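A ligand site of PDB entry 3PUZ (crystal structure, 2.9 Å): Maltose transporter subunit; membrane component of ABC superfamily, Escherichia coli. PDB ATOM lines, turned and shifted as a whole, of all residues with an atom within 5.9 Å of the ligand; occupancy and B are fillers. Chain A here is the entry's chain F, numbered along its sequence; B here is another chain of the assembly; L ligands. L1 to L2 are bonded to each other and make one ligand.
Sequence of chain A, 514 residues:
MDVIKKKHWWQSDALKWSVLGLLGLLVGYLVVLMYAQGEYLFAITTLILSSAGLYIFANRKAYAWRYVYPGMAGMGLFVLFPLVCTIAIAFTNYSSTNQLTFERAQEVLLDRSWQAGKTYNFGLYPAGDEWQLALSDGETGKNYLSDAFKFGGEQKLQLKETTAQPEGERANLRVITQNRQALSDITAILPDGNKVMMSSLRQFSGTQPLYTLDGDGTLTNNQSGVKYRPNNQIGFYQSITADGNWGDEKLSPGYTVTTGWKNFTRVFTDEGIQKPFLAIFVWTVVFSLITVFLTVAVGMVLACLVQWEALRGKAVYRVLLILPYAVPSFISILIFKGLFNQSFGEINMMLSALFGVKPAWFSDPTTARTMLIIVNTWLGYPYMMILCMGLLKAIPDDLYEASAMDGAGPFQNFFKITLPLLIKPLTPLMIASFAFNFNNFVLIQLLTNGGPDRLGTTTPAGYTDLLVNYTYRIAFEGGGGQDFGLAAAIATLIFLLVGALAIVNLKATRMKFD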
ATOM      1  N   THR A 291       9.005  -5.454  25.213  1.00  0.00           N
ATOM      2  CA  THR A 291      10.226  -5.907  25.873  1.00  0.00           C
ATOM      3  C   THR A 291      10.613  -4.955  27.009  1.00  0.00           C
ATOM      4  O   THR A 291      10.744  -5.380  28.158  1.00  0.00           O
ATOM      5  CB  THR A 291      11.400  -6.056  24.880  1.00  0.00           C
ATOM      6  OG1 THR A 291      11.053  -7.005  23.861  1.00  0.00           O
ATOM      7  CG2 THR A 291      12.648  -6.538  25.601  1.00  0.00           C
ATOM      8  N   THR A 295      10.379  -6.073  31.000  1.00  0.00           N
ATOM      9  CA  THR A 295      11.681  -6.190  31.649  1.00  0.00           C
ATOM     10  C   THR A 295      11.885  -5.149  32.756  1.00  0.00           C
ATOM     11  O   THR A 295      12.464  -5.463  33.791  1.00  0.00           O
ATOM     12  CB  THR A 295      12.857  -6.123  30.635  1.00  0.00           C
ATOM     13  OG1 THR A 295      12.760  -4.938  29.846  1.00  0.00           O
ATOM     14  CG2 THR A 295      12.850  -7.345  29.721  1.00  0.00           C
ATOM     15  N   TYR A 325      21.807 -13.906  33.538  1.00  0.00           N
ATOM     16  CA  TYR A 325      22.710 -12.953  32.899  1.00  0.00           C
ATOM     17  C   TYR A 325      24.146 -13.473  32.823  1.00  0.00           C
ATOM     18  O   TYR A 325      24.930 -13.043  31.985  1.00  0.00           O
ATOM     19  CB  TYR A 325      22.657 -11.599  33.625  1.00  0.00           C
ATOM     20  CG  TYR A 325      22.851 -10.374  32.756  1.00  0.00           C
ATOM     21  CD1 TYR A 325      22.526 -10.396  31.395  1.00  0.00           C
ATOM     22  CD2 TYR A 325      23.301  -9.181  33.301  1.00  0.00           C
ATOM     23  CE1 TYR A 325      22.695  -9.264  30.595  1.00  0.00           C
ATOM     24  CE2 TYR A 325      23.463  -8.033  32.519  1.00  0.00           C
ATOM     25  CZ  TYR A 325      23.152  -8.093  31.168  1.00  0.00           C
ATOM     26  OH  TYR A 325      23.309  -6.977  30.383  1.00  0.00           O
ATOM     27  N   SER A 329      23.985 -14.864  26.021  1.00  0.00           N
ATOM     28  CA  SER A 329      22.683 -14.750  25.336  1.00  0.00           C
ATOM     29  C   SER A 329      22.475 -15.860  24.313  1.00  0.00           C
ATOM     30  O   SER A 329      21.446 -16.523  24.317  1.00  0.00           O
ATOM     31  CB  SER A 329      22.533 -13.390  24.668  1.00  0.00           C
ATOM     32  OG  SER A 329      22.833 -12.332  25.558  1.00  0.00           O
ATOM     33  N   ASN A 376      12.730 -13.126  25.644  1.00  0.00           N
ATOM     34  CA  ASN A 376      13.429 -11.845  25.778  1.00  0.00           C
ATOM     35  C   ASN A 376      13.289 -11.254  27.171  1.00  0.00           C
ATOM     36  O   ASN A 376      14.227 -10.641  27.669  1.00  0.00           O
ATOM     37  CB  ASN A 376      12.971 -10.852  24.710  1.00  0.00           C
ATOM     38  CG  ASN A 376      14.073  -9.882  24.297  1.00  0.00           C
ATOM     39  OD1 ASN A 376      15.244 -10.065  24.624  1.00  0.00           O
ATOM     40  ND2 ASN A 376      13.690  -8.851  23.566  1.00  0.00           N
ATOM     41  N   LEU A 379      15.581 -13.031  29.221  1.00  0.00           N
ATOM     42  CA  LEU A 379      16.902 -12.536  28.865  1.00  0.00           C
ATOM     43  C   LEU A 379      17.188 -11.149  29.411  1.00  0.00           C
ATOM     44  O   LEU A 379      18.336 -10.820  29.713  1.00  0.00           O
ATOM     45  CB  LEU A 379      17.057 -12.520  27.337  1.00  0.00           C
ATOM     46  CG  LEU A 379      17.881 -13.608  26.652  1.00  0.00           C
ATOM     47  CD1 LEU A 379      17.287 -14.977  26.817  1.00  0.00           C
ATOM     48  CD2 LEU A 379      18.030 -13.267  25.185  1.00  0.00           C
ATOM     49  N   GLY A 380      16.134 -10.345  29.536  1.00  0.00           N
ATOM     50  CA  GLY A 380      16.290  -8.904  29.770  1.00  0.00           C
ATOM     51  C   GLY A 380      16.001  -8.368  31.157  1.00  0.00           C
ATOM     52  O   GLY A 380      16.369  -7.223  31.460  1.00  0.00           O
ATOM     53  N   TYR A 381      15.361  -9.168  31.998  1.00  0.00           N
ATOM     54  CA  TYR A 381      15.024  -8.734  33.348  1.00  0.00           C
ATOM     55  C   TYR A 381      16.243  -8.540  34.264  1.00  0.00           C
ATOM     56  O   TYR A 381      16.251  -7.613  35.067  1.00  0.00           O
ATOM     57  CB  TYR A 381      13.950  -9.632  34.004  1.00  0.00           C
ATOM     58  CG  TYR A 381      14.497 -10.855  34.734  1.00  0.00           C
ATOM     59  CD1 TYR A 381      15.025 -10.731  36.029  1.00  0.00           C
ATOM     60  CD2 TYR A 381      14.477 -12.111  34.137  1.00  0.00           C
ATOM     61  CE1 TYR A 381      15.532 -11.843  36.696  1.00  0.00           C
ATOM     62  CE2 TYR A 381      14.985 -13.224  34.804  1.00  0.00           C
ATOM     63  CZ  TYR A 381      15.506 -13.087  36.082  1.00  0.00           C
ATOM     64  OH  TYR A 381      16.005 -14.186  36.745  1.00  0.00           O
ATOM     65  N   TYR A 383      19.193  -7.367  33.699  1.00  0.00           N
ATOM     66  CA  TYR A 383      19.814  -6.074  33.436  1.00  0.00           C
ATOM     67  C   TYR A 383      19.027  -4.909  34.042  1.00  0.00           C
ATOM     68  O   TYR A 383      19.612  -3.965  34.546  1.00  0.00           O
ATOM     69  CB  TYR A 383      20.016  -5.880  31.923  1.00  0.00           C
ATOM     70  CG  TYR A 383      20.369  -4.471  31.486  1.00  0.00           C
ATOM     71  CD1 TYR A 383      21.617  -3.914  31.769  1.00  0.00           C
ATOM     72  CD2 TYR A 383      19.450  -3.706  30.775  1.00  0.00           C
ATOM     73  CE1 TYR A 383      21.935  -2.630  31.353  1.00  0.00           C
ATOM     74  CE2 TYR A 383      19.768  -2.412  30.349  1.00  0.00           C
ATOM     75  CZ  TYR A 383      21.001  -1.880  30.649  1.00  0.00           C
ATOM     76  OH  TYR A 383      21.299  -0.610  30.231  1.00  0.00           O
ATOM     77  N   MET A 384      17.700  -4.996  33.992  1.00  0.00           N
ATOM     78  CA  MET A 384      16.836  -3.965  34.562  1.00  0.00           C
ATOM     79  C   MET A 384      16.836  -4.028  36.084  1.00  0.00           C
ATOM     80  O   MET A 384      16.740  -2.990  36.745  1.00  0.00           O
ATOM     81  CB  MET A 384      15.410  -4.070  34.028  1.00  0.00           C
ATOM     82  CG  MET A 384      15.288  -3.831  32.525  1.00  0.00           C
ATOM     83  SD  MET A 384      15.280  -2.094  32.005  1.00  0.00           S
ATOM     84  CE  MET A 384      16.988  -1.604  32.208  1.00  0.00           C
ATOM     85  N   LEU A 429      17.729   5.271  29.919  1.00  0.00           N
ATOM     86  CA  LEU A 429      18.238   3.911  29.839  1.00  0.00           C
ATOM     87  C   LEU A 429      17.248   2.977  29.151  1.00  0.00           C
ATOM     88  O   LEU A 429      17.648   1.993  28.534  1.00  0.00           O
ATOM     89  CB  LEU A 429      18.623   3.393  31.222  1.00  0.00           C
ATOM     90  CG  LEU A 429      19.992   3.868  31.689  1.00  0.00           C
ATOM     91  CD1 LEU A 429      19.985   4.178  33.177  1.00  0.00           C
ATOM     92  CD2 LEU A 429      21.083   2.863  31.321  1.00  0.00           C
ATOM     93  N   ALA A 432      17.120   3.787  25.469  1.00  0.00           N
ATOM     94  CA  ALA A 432      18.292   3.097  24.969  1.00  0.00           C
ATOM     95  C   ALA A 432      17.986   1.617  24.792  1.00  0.00           C
ATOM     96  O   ALA A 432      18.459   0.992  23.844  1.00  0.00           O
ATOM     97  CB  ALA A 432      19.483   3.293  25.901  1.00  0.00           C
ATOM     98  N   SER A 433      17.194   1.066  25.707  1.00  0.00           N
ATOM     99  CA  SER A 433      16.771  -0.332  25.626  1.00  0.00           C
ATOM    100  C   SER A 433      15.883  -0.565  24.416  1.00  0.00           C
ATOM    101  O   SER A 433      15.931  -1.633  23.802  1.00  0.00           O
ATOM    102  CB  SER A 433      16.026  -0.756  26.887  1.00  0.00           C
ATOM    103  OG  SER A 433      15.507  -2.062  26.749  1.00  0.00           O
ATOM    104  N   PHE A 434      15.073   0.434  24.081  1.00  0.00           N
ATOM    105  CA  PHE A 434      14.224   0.394  22.883  1.00  0.00           C
ATOM    106  C   PHE A 434      15.079   0.353  21.627  1.00  0.00           C
ATOM    107  O   PHE A 434      14.765  -0.374  20.687  1.00  0.00           O
ATOM    108  CB  PHE A 434      13.288   1.604  22.846  1.00  0.00           C
ATOM    109  CG  PHE A 434      12.397   1.648  21.641  1.00  0.00           C
ATOM    110  CD1 PHE A 434      12.765   2.391  20.514  1.00  0.00           C
ATOM    111  CD2 PHE A 434      11.193   0.951  21.623  1.00  0.00           C
ATOM    112  CE1 PHE A 434      11.940   2.434  19.388  1.00  0.00           C
ATOM    113  CE2 PHE A 434      10.359   0.997  20.501  1.00  0.00           C
ATOM    114  CZ  PHE A 434      10.733   1.739  19.384  1.00  0.00           C
ATOM    115  N   PHE A 436      18.251  -0.751  21.503  1.00  0.00           N
ATOM    116  CA  PHE A 436      18.909  -2.060  21.509  1.00  0.00           C
ATOM    117  C   PHE A 436      17.957  -3.121  20.952  1.00  0.00           C
ATOM    118  O   PHE A 436      18.269  -3.778  19.963  1.00  0.00           O
ATOM    119  CB  PHE A 436      19.358  -2.439  22.925  1.00  0.00           C
ATOM    120  CG  PHE A 436      19.995  -3.799  23.016  1.00  0.00           C
ATOM    121  CD1 PHE A 436      19.224  -4.926  23.302  1.00  0.00           C
ATOM    122  CD2 PHE A 436      21.362  -3.958  22.823  1.00  0.00           C
ATOM    123  CE1 PHE A 436      19.816  -6.188  23.390  1.00  0.00           C
ATOM    124  CE2 PHE A 436      21.958  -5.211  22.910  1.00  0.00           C
ATOM    125  CZ  PHE A 436      21.174  -6.333  23.192  1.00  0.00           C
ATOM    126  N   ASN A 437      16.794  -3.247  21.584  1.00  0.00           N
ATOM    127  CA  ASN A 437      15.808  -4.256  21.209  1.00  0.00           C
ATOM    128  C   ASN A 437      15.140  -4.016  19.861  1.00  0.00           C
ATOM    129  O   ASN A 437      14.520  -4.927  19.301  1.00  0.00           O
ATOM    130  CB  ASN A 437      14.759  -4.416  22.308  1.00  0.00           C
ATOM    131  CG  ASN A 437      15.279  -5.207  23.493  1.00  0.00           C
ATOM    132  OD1 ASN A 437      15.373  -4.687  24.607  1.00  0.00           O
ATOM    133  ND2 ASN A 437      15.628  -6.466  23.254  1.00  0.00           N
ATOM    134  N   ASN A 440      17.622  -6.015  17.779  1.00  0.00           N
ATOM    135  CA  ASN A 440      18.039  -7.256  18.406  1.00  0.00           C
ATOM    136  C   ASN A 440      18.047  -8.374  17.361  1.00  0.00           C
ATOM    137  O   ASN A 440      17.091  -9.145  17.244  1.00  0.00           O
ATOM    138  CB  ASN A 440      17.131  -7.613  19.587  1.00  0.00           C
ATOM    139  CG  ASN A 440      17.850  -8.401  20.680  1.00  0.00           C
ATOM    140  OD1 ASN A 440      17.693  -8.115  21.864  1.00  0.00           O
ATOM    141  ND2 ASN A 440      18.655  -9.392  20.281  1.00  0.00           N
ATOM    142  N   LEU A 443      18.708 -12.500  18.601  1.00  0.00           N
ATOM    143  CA  LEU A 443      17.564 -13.220  19.177  1.00  0.00           C
ATOM    144  C   LEU A 443      16.701 -13.849  18.082  1.00  0.00           C
ATOM    145  O   LEU A 443      16.360 -15.029  18.155  1.00  0.00           O
ATOM    146  CB  LEU A 443      16.712 -12.311  20.068  1.00  0.00           C
ATOM    147  CG  LEU A 443      15.495 -12.970  20.721  1.00  0.00           C
ATOM    148  CD1 LEU A 443      15.909 -14.012  21.759  1.00  0.00           C
ATOM    149  CD2 LEU A 443      14.579 -11.945  21.354  1.00  0.00           C
ATOM    150  N   LEU B 172      27.135   5.090  24.564  1.00  0.00           N
ATOM    151  CA  LEU B 172      26.212   4.763  25.642  1.00  0.00           C
ATOM    152  C   LEU B 172      26.912   4.935  26.986  1.00  0.00           C
ATOM    153  O   LEU B 172      26.421   5.630  27.875  1.00  0.00           O
ATOM    154  CB  LEU B 172      25.690   3.328  25.518  1.00  0.00           C
ATOM    155  CG  LEU B 172      25.590   2.698  24.107  1.00  0.00           C
ATOM    156  CD1 LEU B 172      25.491   1.169  24.176  1.00  0.00           C
ATOM    157  CD2 LEU B 172      24.441   3.302  23.267  1.00  0.00           C
ATOM    158  N   LEU B 221      29.293  -4.901  32.060  1.00  0.00           N
ATOM    159  CA  LEU B 221      28.375  -4.763  30.921  1.00  0.00           C
ATOM    160  C   LEU B 221      29.083  -4.965  29.582  1.00  0.00           C
ATOM    161  O   LEU B 221      28.597  -5.708  28.728  1.00  0.00           O
ATOM    162  CB  LEU B 221      27.644  -3.418  30.952  1.00  0.00           C
ATOM    163  CG  LEU B 221      26.555  -3.268  32.013  1.00  0.00           C
ATOM    164  CD1 LEU B 221      25.994  -1.849  31.992  1.00  0.00           C
ATOM    165  CD2 LEU B 221      25.427  -4.287  31.823  1.00  0.00           C
ATOM    166  N   ILE B 224      30.159  -8.695  29.187  1.00  0.00           N
ATOM    167  CA  ILE B 224      29.007  -9.500  28.803  1.00  0.00           C
ATOM    168  C   ILE B 224      28.699  -9.276  27.324  1.00  0.00           C
ATOM    169  O   ILE B 224      28.491 -10.231  26.575  1.00  0.00           O
ATOM    170  CB  ILE B 224      27.763  -9.176  29.680  1.00  0.00           C
ATOM    171  CG1 ILE B 224      27.976  -9.680  31.106  1.00  0.00           C
ATOM    172  CG2 ILE B 224      26.491  -9.770  29.076  1.00  0.00           C
ATOM    173  CD1 ILE B 224      27.081  -9.003  32.146  1.00  0.00           C
ATOM    174  N   ALA B 225      28.690  -8.012  26.920  1.00  0.00           N
ATOM    175  CA  ALA B 225      28.373  -7.610  25.548  1.00  0.00           C
ATOM    176  C   ALA B 225      29.264  -8.306  24.519  1.00  0.00           C
ATOM    177  O   ALA B 225      28.779  -8.736  23.473  1.00  0.00           O
ATOM    178  CB  ALA B 225      28.453  -6.100  25.405  1.00  0.00           C
ATOM    179  N   THR B 228      28.933 -12.393  24.096  1.00  0.00           N
ATOM    180  CA  THR B 228      27.796 -12.885  23.327  1.00  0.00           C
ATOM    181  C   THR B 228      27.659 -12.303  21.916  1.00  0.00           C
ATOM    182  O   THR B 228      26.714 -12.646  21.189  1.00  0.00           O
ATOM    183  CB  THR B 228      26.458 -12.755  24.130  1.00  0.00           C
ATOM    184  OG1 THR B 228      25.407 -13.424  23.407  1.00  0.00           O
ATOM    185  CG2 THR B 228      26.084 -11.300  24.359  1.00  0.00           C
HETATM  186  C1  LIG L   1      22.564  -2.820  27.170  1.00  0.00           C
HETATM  187  C2  LIG L   1      23.331  -4.091  27.564  1.00  0.00           C
HETATM  188  C3  LIG L   1      22.704  -5.372  27.013  1.00  0.00           C
HETATM  189  C4  LIG L   1      21.207  -5.414  27.259  1.00  0.00           C
HETATM  190  C5  LIG L   1      20.553  -4.152  26.692  1.00  0.00           C
HETATM  191  C6  LIG L   1      19.034  -4.167  26.884  1.00  0.00           C
HETATM  192  O1  LIG L   1      22.896  -2.383  25.848  1.00  0.00           O
HETATM  193  O2  LIG L   1      24.701  -4.028  27.152  1.00  0.00           O
HETATM  194  O3  LIG L   1      23.303  -6.494  27.649  1.00  0.00           O
HETATM  195  O4  LIG L   1      20.668  -6.596  26.650  1.00  0.00           O
HETATM  196  O5  LIG L   1      21.132  -2.978  27.287  1.00  0.00           O
HETATM  197  O6  LIG L   1      18.544  -2.886  27.303  1.00  0.00           O
HETATM  198  C1  LG2 L   2      20.114  -7.512  27.608  1.00  0.00           C
HETATM  199  C2  LG2 L   2      20.614  -8.926  27.360  1.00  0.00           C
HETATM  200  C3  LG2 L   2      19.985  -9.560  26.116  1.00  0.00           C
HETATM  201  C4  LG2 L   2      18.496  -9.277  25.957  1.00  0.00           C
HETATM  202  C5  LG2 L   2      18.126  -7.828  26.276  1.00  0.00           C
HETATM  203  C6  LG2 L   2      16.609  -7.625  26.331  1.00  0.00           C
HETATM  204  O1  LG2 L   2      22.039  -8.898  27.213  1.00  0.00           O
HETATM  205  O2  LG2 L   2      20.177 -10.977  26.187  1.00  0.00           O
HETATM  206  O3  LG2 L   2      18.122  -9.562  24.602  1.00  0.00           O
HETATM  207  O4  LG2 L   2      18.683  -7.467  27.538  1.00  0.00           O
HETATM  208  O5  LG2 L   2      16.290  -6.390  26.980  1.00  0.00           O
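ND2 of Asn 376 sits close to ND2 of Asn 437 (3.1 Å). ND2 of Asn 376 sits at hydrogen-bond distance from OG1 of Thr 291 (3.2 Å). The backbone NH (N) of Ser 329 lies close to the side-chain hydroxyl (OG1) of Thr 228 of chain B (3.3 Å). ND2 of Asn 437 lies within hydrogen-bond range of OD1 of Asn 440 (3.0 Å). The side-chain amide oxygen (OD1) of Asn 437 sits close to the backbone carbonyl oxygen (O) of Ser 433. OG1 of Thr 295 sits at hydrogen-bond distance from O of Thr 291 (2.7 Å).
CG2 of Thr 291 touches O5 of LG2 L2, at 3.9 Å. Leu 379 touches the ligand. CA of Gly 380 touches O4 of LG2 L2, 3.6 Å away. Tyr 383 touches the ligand. CE1 of Phe 436 touches O4 of LIG L1 (3.4 Å). Hydrophobic or aromatic side chains that line the ligand: Tyr 325, Leu 379, Tyr 383 and Phe 436. Within 4 Å of the ligand: Thr 291, Tyr 325, Ser 329, Asn 376, Leu 379, Gly 380, Tyr 383, Ser 433, Phe 436, Asn 437 and Asn 440.
An oxygen (O3) of LIG L1 is in hydrogen-bond range of the side-chain hydroxyl of Tyr 325, 2.8 Å away. OD1 of Asn 376 sits at hydrogen-bond distance from O3 of LG2 L2 (2.9 Å). O2 of LG2 L2 is in hydrogen-bond range of OG of Ser 329 (3.0 Å). OD1 of Asn 437 sits at hydrogen-bond distance from O5 of LG2 L2, at 3.1 Å. OD1 of Asn 440 is in hydrogen-bond range of O3 of LG2 L2, 3.1 Å away. O6 of LIG L1 lies within hydrogen-bond range of OG of Ser 433.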
